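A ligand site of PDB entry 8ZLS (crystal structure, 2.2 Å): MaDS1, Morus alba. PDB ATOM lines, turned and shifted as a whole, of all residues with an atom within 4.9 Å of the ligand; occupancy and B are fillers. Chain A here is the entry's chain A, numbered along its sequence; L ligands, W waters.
Water W4 lies within hydrogen-bond range of O11 of the ligand (2.7 Å) and OD1 of Asp 90 (2.8 Å).
Water W6 lies within hydrogen-bond range of O of Asn 456 (2.7 Å), O10 of the ligand (2.8 Å) and N of Tyr 91 (3.0 Å).
Water W1 lies within hydrogen-bond range of O of Leu 94 (2.9 Å), O5 of the ligand (2.9 Å) and ND2 of Asn 510 (3.0 Å).
Water W5 bridges the backbone carbonyl oxygen of Gly 158 and an oxygen (O4) of the ligand.
Water W2 bridges the backbone NH (N) of Thr 84 (2.8 Å) and an oxygen (O6) of the ligand (3.1 Å).
O15 of the ligand is in hydrogen-bond range of N of His 89.
The backbone carbonyl oxygen (O) of His 89 is in hydrogen-bond range of an oxygen (O10) of the ligand.
A ring nitrogen (ND1) of His 89 is covalently linked to a carbon (C19) of the ligand, at 1.4 Å.
The side-chain sulfur of Cys 151 is covalently linked to a carbon (C15) of the ligand (1.8 Å).
OG of Ser 95 sits at hydrogen-bond distance from O1 of the ligand, 2.6 Å away.
The side-chain hydroxyl (OH) of Tyr 454 is in hydrogen-bond range of an oxygen (O7) of the ligand.
The backbone carbonyl oxygen of Thr 84 is in hydrogen-bond range of an oxygen (O6) of the ligand (2.7 Å).
The backbone NH (N) of Ser 86 lies within hydrogen-bond range of an oxygen (O2) of the ligand (2.8 Å).
The side-chain hydroxyl (OG) of Ser 86 sits close to an oxygen (O13) of the ligand (3.5 Å).
The backbone NH (N) of Val 216 lies within hydrogen-bond range of a nitrogen (N4) of the ligand, 3.0 Å away.
O of Val 216 sits at hydrogen-bond distance from N3 of the ligand (2.8 Å).
The backbone NH of Gly 155 sits at hydrogen-bond distance from an oxygen (O14) of the ligand, at 2.9 Å.
An oxygen (O2) of the ligand sits at hydrogen-bond distance from the backbone NH (N) of Gly 88 (2.9 Å).
O13 of the ligand is in hydrogen-bond range of N of Gly 87, at 3.0 Å.
The backbone NH of Tyr 165 lies within hydrogen-bond range of an oxygen (O7) of the ligand, at 3.0 Å.
A nitrogen (N7) of the ligand sits at hydrogen-bond distance from the backbone carbonyl oxygen of Tyr 165, at 3.0 Å.
O1 of the ligand lies within hydrogen-bond range of N of Asp 90.
The side-chain amide nitrogen of Gln 159 is in hydrogen-bond range of an oxygen (O9) of the ligand, at 3.2 Å.
The backbone NH (N) of Asp 150 sits at hydrogen-bond distance from an oxygen (O8) of the ligand, 3.2 Å away.
An oxygen (O13) of the ligand sits at hydrogen-bond distance from the backbone NH (N) of Gly 158 (3.2 Å).
An oxygen (O11) of the ligand sits at hydrogen-bond distance from the backbone carbonyl oxygen (O) of Gly 158 (3.4 Å).
The backbone carbonyl oxygen (O) of Asn 456 sits at hydrogen-bond distance from an oxygen (O10) of the ligand (3.5 Å).
OD1 of Asn 456 is in hydrogen-bond range of O11 of the ligand.
An oxygen (O5) of the ligand lies within hydrogen-bond range of the guanidinium group (NH2) of Arg 458.
The side-chain hydroxyl (OH) of Tyr 454 is in hydrogen-bond range of the backbone NH (N) of Gly 164 (2.9 Å).
The backbone carbonyl oxygen (O) of Ala 126 sits at hydrogen-bond distance from the side-chain hydroxyl (OG) of Ser 86 (2.8 Å).
The side-chain carboxylate of Asp 90 lies within salt-bridge range of the guanidinium group of Arg 458, 2.9 Å away.
The side-chain carboxylate (OD2) of Asp 90 is in hydrogen-bond range of the backbone NH (N) of Leu 94 (3.0 Å).
N of Gly 149 lies within hydrogen-bond range of OE1 of Gln 159 (2.6 Å).
The backbone NH of Gly 164 lies within hydrogen-bond range of the backbone carbonyl oxygen of Gln 159, at 3.3 Å.
The backbone carbonyl oxygen of Gly 158 lies close to the side-chain amide oxygen of Asn 456, at 3.3 Å.
O of Ala 126 sits at hydrogen-bond distance from N of Gly 157, at 3.3 Å.
Merely in contact with the ligand: Arg 85 (3.7 Å), Tyr 91 (3.99 Å), Leu 107 (3.1 Å), Ala 126 (3.6 Å), Gly 149 (3.3 Å), Val 154 (3.8 Å), Gly 157 (3.6 Å), Gly 164 (3.9 Å), Pro 210 (3.7 Å), Ala 211 (3.7 Å), Gly 214 (3.7 Å) and Ile 215 (3.7 Å).
Hydrophobic or aromatic side chains that line the ligand: His 89, Tyr 91, Leu 107, Ala 126, Val 154, Tyr 165, Pro 210, Ala 211, Val 216 and Tyr 454.
Along chain A the residues within 4 Å of the ligand span positions 84 to 458.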
ATOM      1  N   THR A  84      20.310  21.741  14.441  1.00  0.00           N
ATOM      2  CA  THR A  84      18.887  21.478  14.538  1.00  0.00           C
ATOM      3  C   THR A  84      18.136  22.785  14.363  1.00  0.00           C
ATOM      4  O   THR A  84      18.465  23.797  14.992  1.00  0.00           O
ATOM      5  CB  THR A  84      18.546  20.842  15.887  1.00  0.00           C
ATOM      6  OG1 THR A  84      19.225  19.582  16.003  1.00  0.00           O
ATOM      7  CG2 THR A  84      17.017  20.604  16.022  1.00  0.00           C
ATOM      8  N   ARG A  85      17.116  22.775  13.518  1.00  0.00           N
ATOM      9  CA  ARG A  85      16.310  23.966  13.327  1.00  0.00           C
ATOM     10  C   ARG A  85      14.845  23.634  13.559  1.00  0.00           C
ATOM     11  O   ARG A  85      14.313  22.696  12.979  1.00  0.00           O
ATOM     12  CB  ARG A  85      16.510  24.556  11.946  1.00  0.00           C
ATOM     13  CG  ARG A  85      15.893  25.922  11.813  1.00  0.00           C
ATOM     14  CD  ARG A  85      16.429  26.637  10.576  1.00  0.00           C
ATOM     15  NE  ARG A  85      15.955  26.005   9.356  1.00  0.00           N
ATOM     16  CZ  ARG A  85      16.089  26.537   8.142  1.00  0.00           C
ATOM     17  NH1 ARG A  85      16.729  27.687   7.959  1.00  0.00           N
ATOM     18  NH2 ARG A  85      15.548  25.924   7.099  1.00  0.00           N
ATOM     19  N   SER A  86      14.198  24.433  14.401  1.00  0.00           N
ATOM     20  CA  SER A  86      12.774  24.310  14.650  1.00  0.00           C
ATOM     21  C   SER A  86      12.031  25.503  14.035  1.00  0.00           C
ATOM     22  O   SER A  86      11.407  25.345  12.999  1.00  0.00           O
ATOM     23  CB  SER A  86      12.516  24.205  16.159  1.00  0.00           C
ATOM     24  OG  SER A  86      11.153  24.326  16.456  1.00  0.00           O
ATOM     25  N   GLY A  87      12.138  26.692  14.612  1.00  0.00           N
ATOM     26  CA  GLY A  87      11.473  27.846  14.036  1.00  0.00           C
ATOM     27  C   GLY A  87      12.428  28.758  13.284  1.00  0.00           C
ATOM     28  O   GLY A  87      12.001  29.649  12.551  1.00  0.00           O
ATOM     29  N   GLY A  88      13.721  28.564  13.510  1.00  0.00           N
ATOM     30  CA  GLY A  88      14.723  29.381  12.855  1.00  0.00           C
ATOM     31  C   GLY A  88      14.788  30.821  13.345  1.00  0.00           C
ATOM     32  O   GLY A  88      15.260  31.692  12.612  1.00  0.00           O
ATOM     33  N   HIS A  89      14.371  31.075  14.573  1.00  0.00           N
ATOM     34  CA  HIS A  89      14.401  32.431  15.102  1.00  0.00           C
ATOM     35  C   HIS A  89      15.669  32.763  15.879  1.00  0.00           C
ATOM     36  O   HIS A  89      15.738  33.835  16.465  1.00  0.00           O
ATOM     37  CB  HIS A  89      13.184  32.678  15.976  1.00  0.00           C
ATOM     38  CG  HIS A  89      12.103  33.401  15.260  1.00  0.00           C
ATOM     39  ND1 HIS A  89      11.968  34.787  15.316  1.00  0.00           N
ATOM     40  CD2 HIS A  89      11.152  32.957  14.413  1.00  0.00           C
ATOM     41  CE1 HIS A  89      10.959  35.130  14.533  1.00  0.00           C
ATOM     42  NE2 HIS A  89      10.433  34.040  13.988  1.00  0.00           N
ATOM     43  N   ASP A  90      16.666  31.884  15.885  1.00  0.00           N
ATOM     44  CA  ASP A  90      17.869  32.155  16.658  1.00  0.00           C
ATOM     45  C   ASP A  90      18.449  33.506  16.246  1.00  0.00           C
ATOM     46  O   ASP A  90      18.633  33.771  15.049  1.00  0.00           O
ATOM     47  CB  ASP A  90      18.888  31.034  16.453  1.00  0.00           C
ATOM     48  CG  ASP A  90      20.084  31.152  17.389  1.00  0.00           C
ATOM     49  OD1 ASP A  90      20.070  30.448  18.433  1.00  0.00           O
ATOM     50  OD2 ASP A  90      21.054  31.889  17.072  1.00  0.00           O
ATOM     51  N   TYR A  91      18.657  34.378  17.254  1.00  0.00           N
ATOM     52  CA  TYR A  91      19.118  35.745  17.018  1.00  0.00           C
ATOM     53  C   TYR A  91      20.427  35.784  16.244  1.00  0.00           C
ATOM     54  O   TYR A  91      20.711  36.753  15.524  1.00  0.00           O
ATOM     55  CB  TYR A  91      19.294  36.467  18.343  1.00  0.00           C
ATOM     56  CG  TYR A  91      18.059  37.123  18.895  1.00  0.00           C
ATOM     57  CD1 TYR A  91      16.780  36.738  18.499  1.00  0.00           C
ATOM     58  CD2 TYR A  91      18.182  38.128  19.833  1.00  0.00           C
ATOM     59  CE1 TYR A  91      15.653  37.353  19.036  1.00  0.00           C
ATOM     60  CE2 TYR A  91      17.072  38.744  20.370  1.00  0.00           C
ATOM     61  CZ  TYR A  91      15.816  38.362  19.966  1.00  0.00           C
ATOM     62  OH  TYR A  91      14.762  39.003  20.534  1.00  0.00           O
ATOM     63  N   LEU A  94      22.186  30.382  14.726  1.00  0.00           N
ATOM     64  CA  LEU A  94      22.945  29.181  15.029  1.00  0.00           C
ATOM     65  C   LEU A  94      22.259  27.903  14.570  1.00  0.00           C
ATOM     66  O   LEU A  94      22.889  26.829  14.598  1.00  0.00           O
ATOM     67  CB  LEU A  94      23.248  29.093  16.535  1.00  0.00           C
ATOM     68  CG  LEU A  94      24.273  30.103  17.058  1.00  0.00           C
ATOM     69  CD1 LEU A  94      24.941  29.603  18.345  1.00  0.00           C
ATOM     70  CD2 LEU A  94      25.310  30.402  15.983  1.00  0.00           C
ATOM     71  N   SER A  95      21.002  27.967  14.181  1.00  0.00           N
ATOM     72  CA  SER A  95      20.315  26.766  13.731  1.00  0.00           C
ATOM     73  C   SER A  95      20.469  26.507  12.239  1.00  0.00           C
ATOM     74  O   SER A  95      19.923  25.520  11.729  1.00  0.00           O
ATOM     75  CB  SER A  95      18.826  26.866  14.095  1.00  0.00           C
ATOM     76  OG  SER A  95      18.288  28.081  13.605  1.00  0.00           O
ATOM     77  N   LEU A 107      12.972  20.537  11.635  1.00  0.00           N
ATOM     78  CA  LEU A 107      11.903  19.767  12.247  1.00  0.00           C
ATOM     79  C   LEU A 107      10.493  20.224  11.844  1.00  0.00           C
ATOM     80  O   LEU A 107       9.529  19.802  12.487  1.00  0.00           O
ATOM     81  CB  LEU A 107      12.033  19.813  13.756  1.00  0.00           C
ATOM     82  CG  LEU A 107      13.420  19.418  14.260  1.00  0.00           C
ATOM     83  CD1 LEU A 107      13.550  19.752  15.730  1.00  0.00           C
ATOM     84  CD2 LEU A 107      13.628  17.936  14.011  1.00  0.00           C
ATOM     85  N   ALA A 126       8.477  18.907  18.442  1.00  0.00           N
ATOM     86  CA  ALA A 126       9.343  20.065  18.670  1.00  0.00           C
ATOM     87  C   ALA A 126       9.451  20.992  17.472  1.00  0.00           C
ATOM     88  O   ALA A 126      10.029  22.076  17.595  1.00  0.00           O
ATOM     89  CB  ALA A 126      10.742  19.605  19.089  1.00  0.00           C
ATOM     90  N   GLY A 149       5.953  32.697  24.526  1.00  0.00           N
ATOM     91  CA  GLY A 149       6.142  34.026  23.955  1.00  0.00           C
ATOM     92  C   GLY A 149       4.916  34.479  23.177  1.00  0.00           C
ATOM     93  O   GLY A 149       3.888  33.801  23.136  1.00  0.00           O
ATOM     94  N   ASP A 150       5.021  35.649  22.537  1.00  0.00           N
ATOM     95  CA  ASP A 150       3.913  36.087  21.694  1.00  0.00           C
ATOM     96  C   ASP A 150       4.242  36.169  20.208  1.00  0.00           C
ATOM     97  O   ASP A 150       3.385  36.566  19.429  1.00  0.00           O
ATOM     98  CB  ASP A 150       3.341  37.450  22.125  1.00  0.00           C
ATOM     99  CG  ASP A 150       4.414  38.481  22.388  1.00  0.00           C
ATOM    100  OD1 ASP A 150       4.436  39.062  23.499  1.00  0.00           O
ATOM    101  OD2 ASP A 150       5.259  38.696  21.487  1.00  0.00           O
ATOM    102  N   CYS A 151       5.456  35.824  19.778  1.00  0.00           N
ATOM    103  CA  CYS A 151       5.754  35.778  18.354  1.00  0.00           C
ATOM    104  C   CYS A 151       5.296  34.424  17.801  1.00  0.00           C
ATOM    105  O   CYS A 151       5.936  33.406  18.103  1.00  0.00           O
ATOM    106  CB  CYS A 151       7.252  35.993  18.095  1.00  0.00           C
ATOM    107  SG  CYS A 151       8.098  37.578  18.631  1.00  0.00           S
ATOM    108  N   GLY A 153       5.430  32.720  15.035  1.00  0.00           N
ATOM    109  CA  GLY A 153       6.284  31.947  14.159  1.00  0.00           C
ATOM    110  C   GLY A 153       7.408  31.192  14.852  1.00  0.00           C
ATOM    111  O   GLY A 153       8.093  30.391  14.210  1.00  0.00           O
ATOM    112  N   VAL A 154       7.610  31.442  16.153  1.00  0.00           N
ATOM    113  CA  VAL A 154       8.719  30.861  16.894  1.00  0.00           C
ATOM    114  C   VAL A 154       8.476  29.377  17.137  1.00  0.00           C
ATOM    115  O   VAL A 154       7.366  28.947  17.475  1.00  0.00           O
ATOM    116  CB  VAL A 154       8.898  31.619  18.226  1.00  0.00           C
ATOM    117  CG1 VAL A 154       9.812  30.846  19.187  1.00  0.00           C
ATOM    118  CG2 VAL A 154       9.416  32.998  17.970  1.00  0.00           C
ATOM    119  N   GLY A 155       9.533  28.575  16.997  1.00  0.00           N
ATOM    120  CA  GLY A 155       9.441  27.144  17.268  1.00  0.00           C
ATOM    121  C   GLY A 155       9.390  26.843  18.767  1.00  0.00           C
ATOM    122  O   GLY A 155      10.072  27.474  19.579  1.00  0.00           O
ATOM    123  N   ILE A 156       8.592  25.833  19.125  1.00  0.00           N
ATOM    124  CA  ILE A 156       8.525  25.381  20.508  1.00  0.00           C
ATOM    125  C   ILE A 156       9.862  24.760  20.925  1.00  0.00           C
ATOM    126  O   ILE A 156      10.218  24.766  22.109  1.00  0.00           O
ATOM    127  CB  ILE A 156       7.356  24.401  20.689  1.00  0.00           C
ATOM    128  CG1 ILE A 156       6.937  24.285  22.156  1.00  0.00           C
ATOM    129  CG2 ILE A 156       7.699  23.025  20.166  1.00  0.00           C
ATOM    130  CD1 ILE A 156       6.070  25.424  22.621  1.00  0.00           C
ATOM    131  N   GLY A 157      10.623  24.225  19.972  1.00  0.00           N
ATOM    132  CA  GLY A 157      11.855  23.536  20.331  1.00  0.00           C
ATOM    133  C   GLY A 157      12.849  24.487  20.961  1.00  0.00           C
ATOM    134  O   GLY A 157      13.329  24.260  22.070  1.00  0.00           O
ATOM    135  N   GLY A 158      13.127  25.597  20.266  1.00  0.00           N
ATOM    136  CA  GLY A 158      14.113  26.527  20.763  1.00  0.00           C
ATOM    137  C   GLY A 158      13.613  27.399  21.893  1.00  0.00           C
ATOM    138  O   GLY A 158      14.391  27.756  22.791  1.00  0.00           O
ATOM    139  N   GLN A 159      12.326  27.772  21.878  1.00  0.00           N
ATOM    140  CA  GLN A 159      11.851  28.717  22.886  1.00  0.00           C
ATOM    141  C   GLN A 159      11.841  28.064  24.261  1.00  0.00           C
ATOM    142  O   GLN A 159      12.327  28.648  25.237  1.00  0.00           O
ATOM    143  CB  GLN A 159      10.473  29.267  22.542  1.00  0.00           C
ATOM    144  CG  GLN A 159      10.023  30.237  23.634  1.00  0.00           C
ATOM    145  CD  GLN A 159       8.959  31.229  23.197  1.00  0.00           C
ATOM    146  OE1 GLN A 159       7.786  31.072  23.523  1.00  0.00           O
ATOM    147  NE2 GLN A 159       9.371  32.267  22.465  1.00  0.00           N
ATOM    148  N   GLY A 164      11.618  30.714  27.731  1.00  0.00           N
ATOM    149  CA  GLY A 164      10.290  30.952  27.189  1.00  0.00           C
ATOM    150  C   GLY A 164       9.460  31.937  28.009  1.00  0.00           C
ATOM    151  O   GLY A 164       8.660  31.529  28.858  1.00  0.00           O
ATOM    152  N   TYR A 165       9.655  33.226  27.758  1.00  0.00           N
ATOM    153  CA  TYR A 165       9.034  34.286  28.551  1.00  0.00           C
ATOM    154  C   TYR A 165       7.842  34.881  27.814  1.00  0.00           C
ATOM    155  O   TYR A 165       7.833  34.963  26.580  1.00  0.00           O
ATOM    156  CB  TYR A 165      10.060  35.386  28.887  1.00  0.00           C
ATOM    157  CG  TYR A 165       9.444  36.621  29.506  1.00  0.00           C
ATOM    158  CD1 TYR A 165       8.960  37.654  28.699  1.00  0.00           C
ATOM    159  CD2 TYR A 165       9.358  36.772  30.873  1.00  0.00           C
ATOM    160  CE1 TYR A 165       8.377  38.775  29.243  1.00  0.00           C
ATOM    161  CE2 TYR A 165       8.799  37.894  31.433  1.00  0.00           C
ATOM    162  CZ  TYR A 165       8.305  38.899  30.616  1.00  0.00           C
ATOM    163  OH  TYR A 165       7.743  40.043  31.165  1.00  0.00           O
ATOM    164  N   PRO A 210      19.175  23.045  24.334  1.00  0.00           N
ATOM    165  CA  PRO A 210      19.253  21.624  23.961  1.00  0.00           C
ATOM    166  C   PRO A 210      20.268  21.324  22.874  1.00  0.00           C
ATOM    167  O   PRO A 210      20.659  20.156  22.731  1.00  0.00           O
ATOM    168  CB  PRO A 210      17.835  21.312  23.474  1.00  0.00           C
ATOM    169  CG  PRO A 210      16.989  22.408  23.961  1.00  0.00           C
ATOM    170  CD  PRO A 210      17.858  23.624  24.050  1.00  0.00           C
ATOM    171  N   ALA A 211      20.691  22.309  22.082  1.00  0.00           N
ATOM    172  CA  ALA A 211      21.619  22.017  20.995  1.00  0.00           C
ATOM    173  C   ALA A 211      22.967  21.533  21.510  1.00  0.00           C
ATOM    174  O   ALA A 211      23.709  20.913  20.757  1.00  0.00           O
ATOM    175  CB  ALA A 211      21.802  23.258  20.111  1.00  0.00           C
ATOM    176  N   GLY A 214      21.724  17.164  22.510  1.00  0.00           N
ATOM    177  CA  GLY A 214      21.052  16.203  21.640  1.00  0.00           C
ATOM    178  C   GLY A 214      19.978  16.926  20.831  1.00  0.00           C
ATOM    179  O   GLY A 214      20.070  18.128  20.594  1.00  0.00           O
ATOM    180  N   ILE A 215      18.948  16.175  20.471  1.00  0.00           N
ATOM    181  CA  ILE A 215      17.868  16.694  19.620  1.00  0.00           C
ATOM    182  C   ILE A 215      16.541  16.382  20.300  1.00  0.00           C
ATOM    183  O   ILE A 215      16.164  15.207  20.422  1.00  0.00           O
ATOM    184  CB  ILE A 215      17.898  16.078  18.221  1.00  0.00           C
ATOM    185  CG1 ILE A 215      19.204  16.510  17.528  1.00  0.00           C
ATOM    186  CG2 ILE A 215      16.649  16.538  17.414  1.00  0.00           C
ATOM    187  CD1 ILE A 215      19.599  15.653  16.361  1.00  0.00           C
ATOM    188  N   VAL A 216      15.833  17.421  20.743  1.00  0.00           N
ATOM    189  CA  VAL A 216      14.526  17.228  21.365  1.00  0.00           C
ATOM    190  C   VAL A 216      13.501  16.949  20.274  1.00  0.00           C
ATOM    191  O   VAL A 216      13.377  17.695  19.296  1.00  0.00           O
ATOM    192  CB  VAL A 216      14.128  18.468  22.191  1.00  0.00           C
ATOM    193  CG1 VAL A 216      12.758  18.268  22.828  1.00  0.00           C
ATOM    194  CG2 VAL A 216      15.166  18.729  23.253  1.00  0.00           C
ATOM    195  N   TYR A 454      19.795  36.791  28.887  1.00  0.00           N
ATOM    196  CA  TYR A 454      18.747  35.807  28.586  1.00  0.00           C
ATOM    197  C   TYR A 454      19.174  34.992  27.361  1.00  0.00           C
ATOM    198  O   TYR A 454      19.419  35.560  26.293  1.00  0.00           O
ATOM    199  CB  TYR A 454      17.424  36.525  28.351  1.00  0.00           C
ATOM    200  CG  TYR A 454      16.213  35.626  28.080  1.00  0.00           C
ATOM    201  CD1 TYR A 454      16.094  34.354  28.635  1.00  0.00           C
ATOM    202  CD2 TYR A 454      15.167  36.082  27.270  1.00  0.00           C
ATOM    203  CE1 TYR A 454      14.957  33.553  28.365  1.00  0.00           C
ATOM    204  CE2 TYR A 454      14.054  35.325  27.012  1.00  0.00           C
ATOM    205  CZ  TYR A 454      13.952  34.061  27.555  1.00  0.00           C
ATOM    206  OH  TYR A 454      12.827  33.328  27.253  1.00  0.00           O
ATOM    207  N   ASN A 456      17.591  33.069  25.327  1.00  0.00           N
ATOM    208  CA  ASN A 456      16.753  33.216  24.136  1.00  0.00           C
ATOM    209  C   ASN A 456      16.992  34.531  23.400  1.00  0.00           C
ATOM    210  O   ASN A 456      16.501  34.681  22.273  1.00  0.00           O
ATOM    211  CB  ASN A 456      15.271  33.081  24.514  1.00  0.00           C
ATOM    212  CG  ASN A 456      14.792  31.624  24.454  1.00  0.00           C
ATOM    213  OD1 ASN A 456      15.448  30.755  23.845  1.00  0.00           O
ATOM    214  ND2 ASN A 456      13.659  31.352  25.093  1.00  0.00           N
ATOM    215  N   PHE A 457      17.685  35.482  23.999  1.00  0.00           N
ATOM    216  CA  PHE A 457      18.203  36.648  23.272  1.00  0.00           C
ATOM    217  C   PHE A 457      19.694  36.437  22.995  1.00  0.00           C
ATOM    218  O   PHE A 457      20.556  37.174  23.479  1.00  0.00           O
ATOM    219  CB  PHE A 457      17.980  37.940  24.057  1.00  0.00           C
ATOM    220  CG  PHE A 457      16.558  38.214  24.441  1.00  0.00           C
ATOM    221  CD1 PHE A 457      15.498  37.749  23.661  1.00  0.00           C
ATOM    222  CD2 PHE A 457      16.283  38.953  25.593  1.00  0.00           C
ATOM    223  CE1 PHE A 457      14.205  37.999  24.023  1.00  0.00           C
ATOM    224  CE2 PHE A 457      14.972  39.208  25.968  1.00  0.00           C
ATOM    225  CZ  PHE A 457      13.924  38.738  25.183  1.00  0.00           C
ATOM    226  N   ARG A 458      19.989  35.406  22.218  1.00  0.00           N
ATOM    227  CA  ARG A 458      21.375  34.975  22.037  1.00  0.00           C
ATOM    228  C   ARG A 458      22.242  36.096  21.469  1.00  0.00           C
ATOM    229  O   ARG A 458      21.808  36.867  20.606  1.00  0.00           O
ATOM    230  CB  ARG A 458      21.453  33.772  21.121  1.00  0.00           C
ATOM    231  CG  ARG A 458      22.703  32.956  21.354  1.00  0.00           C
ATOM    232  CD  ARG A 458      23.044  32.134  20.127  1.00  0.00           C
ATOM    233  NE  ARG A 458      22.365  30.842  20.142  1.00  0.00           N
ATOM    234  CZ  ARG A 458      22.613  29.865  20.996  1.00  0.00           C
ATOM    235  NH1 ARG A 458      23.445  30.033  22.022  1.00  0.00           N
ATOM    236  NH2 ARG A 458      22.019  28.689  20.838  1.00  0.00           N
ATOM    237  N   ASN A 510      28.370  23.942  18.986  1.00  0.00           N
ATOM    238  CA  ASN A 510      28.208  25.137  18.170  1.00  0.00           C
ATOM    239  C   ASN A 510      29.064  26.219  18.815  1.00  0.00           C
ATOM    240  O   ASN A 510      29.822  25.952  19.761  1.00  0.00           O
ATOM    241  CB  ASN A 510      26.731  25.526  17.996  1.00  0.00           C
ATOM    242  CG  ASN A 510      26.027  25.886  19.314  1.00  0.00           C
ATOM    243  OD1 ASN A 510      26.659  26.304  20.301  1.00  0.00           O
ATOM    244  ND2 ASN A 510      24.698  25.764  19.323  1.00  0.00           N
HETATM  245  P1  LIG L   1      15.787  27.996  16.128  1.00  0.00           P
HETATM  246  O1  LIG L   1      16.756  28.938  15.488  1.00  0.00           O
HETATM  247  O2  LIG L   1      15.255  26.874  15.290  1.00  0.00           O
HETATM  248  O3  LIG L   1      16.398  27.270  17.421  1.00  0.00           O
HETATM  249  C1  LIG L   1      17.095  28.032  18.445  1.00  0.00           C
HETATM  250  C2  LIG L   1      18.224  27.234  19.050  1.00  0.00           C
HETATM  251  O4  LIG L   1      17.704  26.038  19.673  1.00  0.00           O
HETATM  252  C3  LIG L   1      19.281  26.761  18.059  1.00  0.00           C
HETATM  253  O5  LIG L   1      20.572  26.686  18.668  1.00  0.00           O
HETATM  254  C4  LIG L   1      18.747  25.385  17.648  1.00  0.00           C
HETATM  255  O6  LIG L   1      19.793  24.538  17.198  1.00  0.00           O
HETATM  256  C5  LIG L   1      18.158  24.888  18.971  1.00  0.00           C
HETATM  257  N1  LIG L   1      17.021  23.990  18.790  1.00  0.00           N
HETATM  258  C6  LIG L   1      15.786  24.298  18.273  1.00  0.00           C
HETATM  259  N2  LIG L   1      14.958  23.281  18.238  1.00  0.00           N
HETATM  260  C7  LIG L   1      15.696  22.234  18.780  1.00  0.00           C
HETATM  261  C8  LIG L   1      15.396  20.881  19.010  1.00  0.00           C
HETATM  262  N3  LIG L   1      14.216  20.319  18.738  1.00  0.00           N
HETATM  263  N4  LIG L   1      16.366  20.116  19.567  1.00  0.00           N
HETATM  264  C9  LIG L   1      17.547  20.670  19.850  1.00  0.00           C
HETATM  265  N5  LIG L   1      17.940  21.935  19.676  1.00  0.00           N
HETATM  266  C10 LIG L   1      16.966  22.671  19.126  1.00  0.00           C
HETATM  267  N6  LIG L   1      11.581  34.654  23.187  1.00  0.00           N
HETATM  268  C11 LIG L   1      10.834  34.774  24.322  1.00  0.00           C
HETATM  269  O7  LIG L   1      11.214  34.277  25.403  1.00  0.00           O
HETATM  270  N7  LIG L   1       9.626  35.468  24.279  1.00  0.00           N
HETATM  271  C12 LIG L   1       9.074  36.081  23.164  1.00  0.00           C
HETATM  272  O8  LIG L   1       7.996  36.664  23.237  1.00  0.00           O
HETATM  273  C13 LIG L   1       9.887  35.949  21.975  1.00  0.00           C
HETATM  274  N8  LIG L   1       9.446  36.476  20.892  1.00  0.00           N
HETATM  275  C14 LIG L   1      10.200  36.337  19.735  1.00  0.00           C
HETATM  276  C15 LIG L   1       9.728  36.904  18.560  1.00  0.00           C
HETATM  277  C16 LIG L   1      10.440  36.792  17.363  1.00  0.00           C
HETATM  278  C17 LIG L   1       9.882  37.434  16.123  1.00  0.00           C
HETATM  279  C18 LIG L   1      11.660  36.096  17.353  1.00  0.00           C
HETATM  280  C19 LIG L   1      12.448  35.918  16.067  1.00  0.00           C
HETATM  281  C20 LIG L   1      12.139  35.522  18.532  1.00  0.00           C
HETATM  282  C21 LIG L   1      11.420  35.648  19.713  1.00  0.00           C
HETATM  283  N9  LIG L   1      11.874  35.085  20.925  1.00  0.00           N
HETATM  284  C22 LIG L   1      11.126  35.217  22.086  1.00  0.00           C
HETATM  285  C23 LIG L   1      13.152  34.367  20.992  1.00  0.00           C
HETATM  286  C24 LIG L   1      13.007  32.867  20.931  1.00  0.00           C
HETATM  287  O9  LIG L   1      12.511  32.367  22.174  1.00  0.00           O
HETATM  288  C25 LIG L   1      14.386  32.245  20.710  1.00  0.00           C
HETATM  289  O10 LIG L   1      15.020  32.944  19.653  1.00  0.00           O
HETATM  290  C26 LIG L   1      14.305  30.767  20.366  1.00  0.00           C
HETATM  291  O11 LIG L   1      15.552  30.132  20.666  1.00  0.00           O
HETATM  292  C27 LIG L   1      13.900  30.545  18.922  1.00  0.00           C
HETATM  293  O12 LIG L   1      13.401  29.199  18.774  1.00  0.00           O
HETATM  294  P2  LIG L   1      13.202  28.566  17.356  1.00  0.00           P
HETATM  295  O13 LIG L   1      12.934  27.125  17.425  1.00  0.00           O
HETATM  296  O14 LIG L   1      12.219  29.449  16.606  1.00  0.00           O
HETATM  297  O15 LIG L   1      14.594  28.845  16.720  1.00  0.00           O
HETATM  298  O   HOH W   1      22.688  25.431  17.109  1.00  0.00           O
HETATM  299  O   HOH W   2      22.018  22.445  16.581  1.00  0.00           O
HETATM  300  O   HOH W   3       7.957  38.783  24.933  1.00  0.00           O
HETATM  301  O   HOH W   4      18.067  31.180  20.322  1.00  0.00           O
HETATM  302  O   HOH W   5      17.190  26.822  22.577  1.00  0.00           O
HETATM  303  O   HOH W   6      17.653  33.780  20.037  1.00  0.00           O
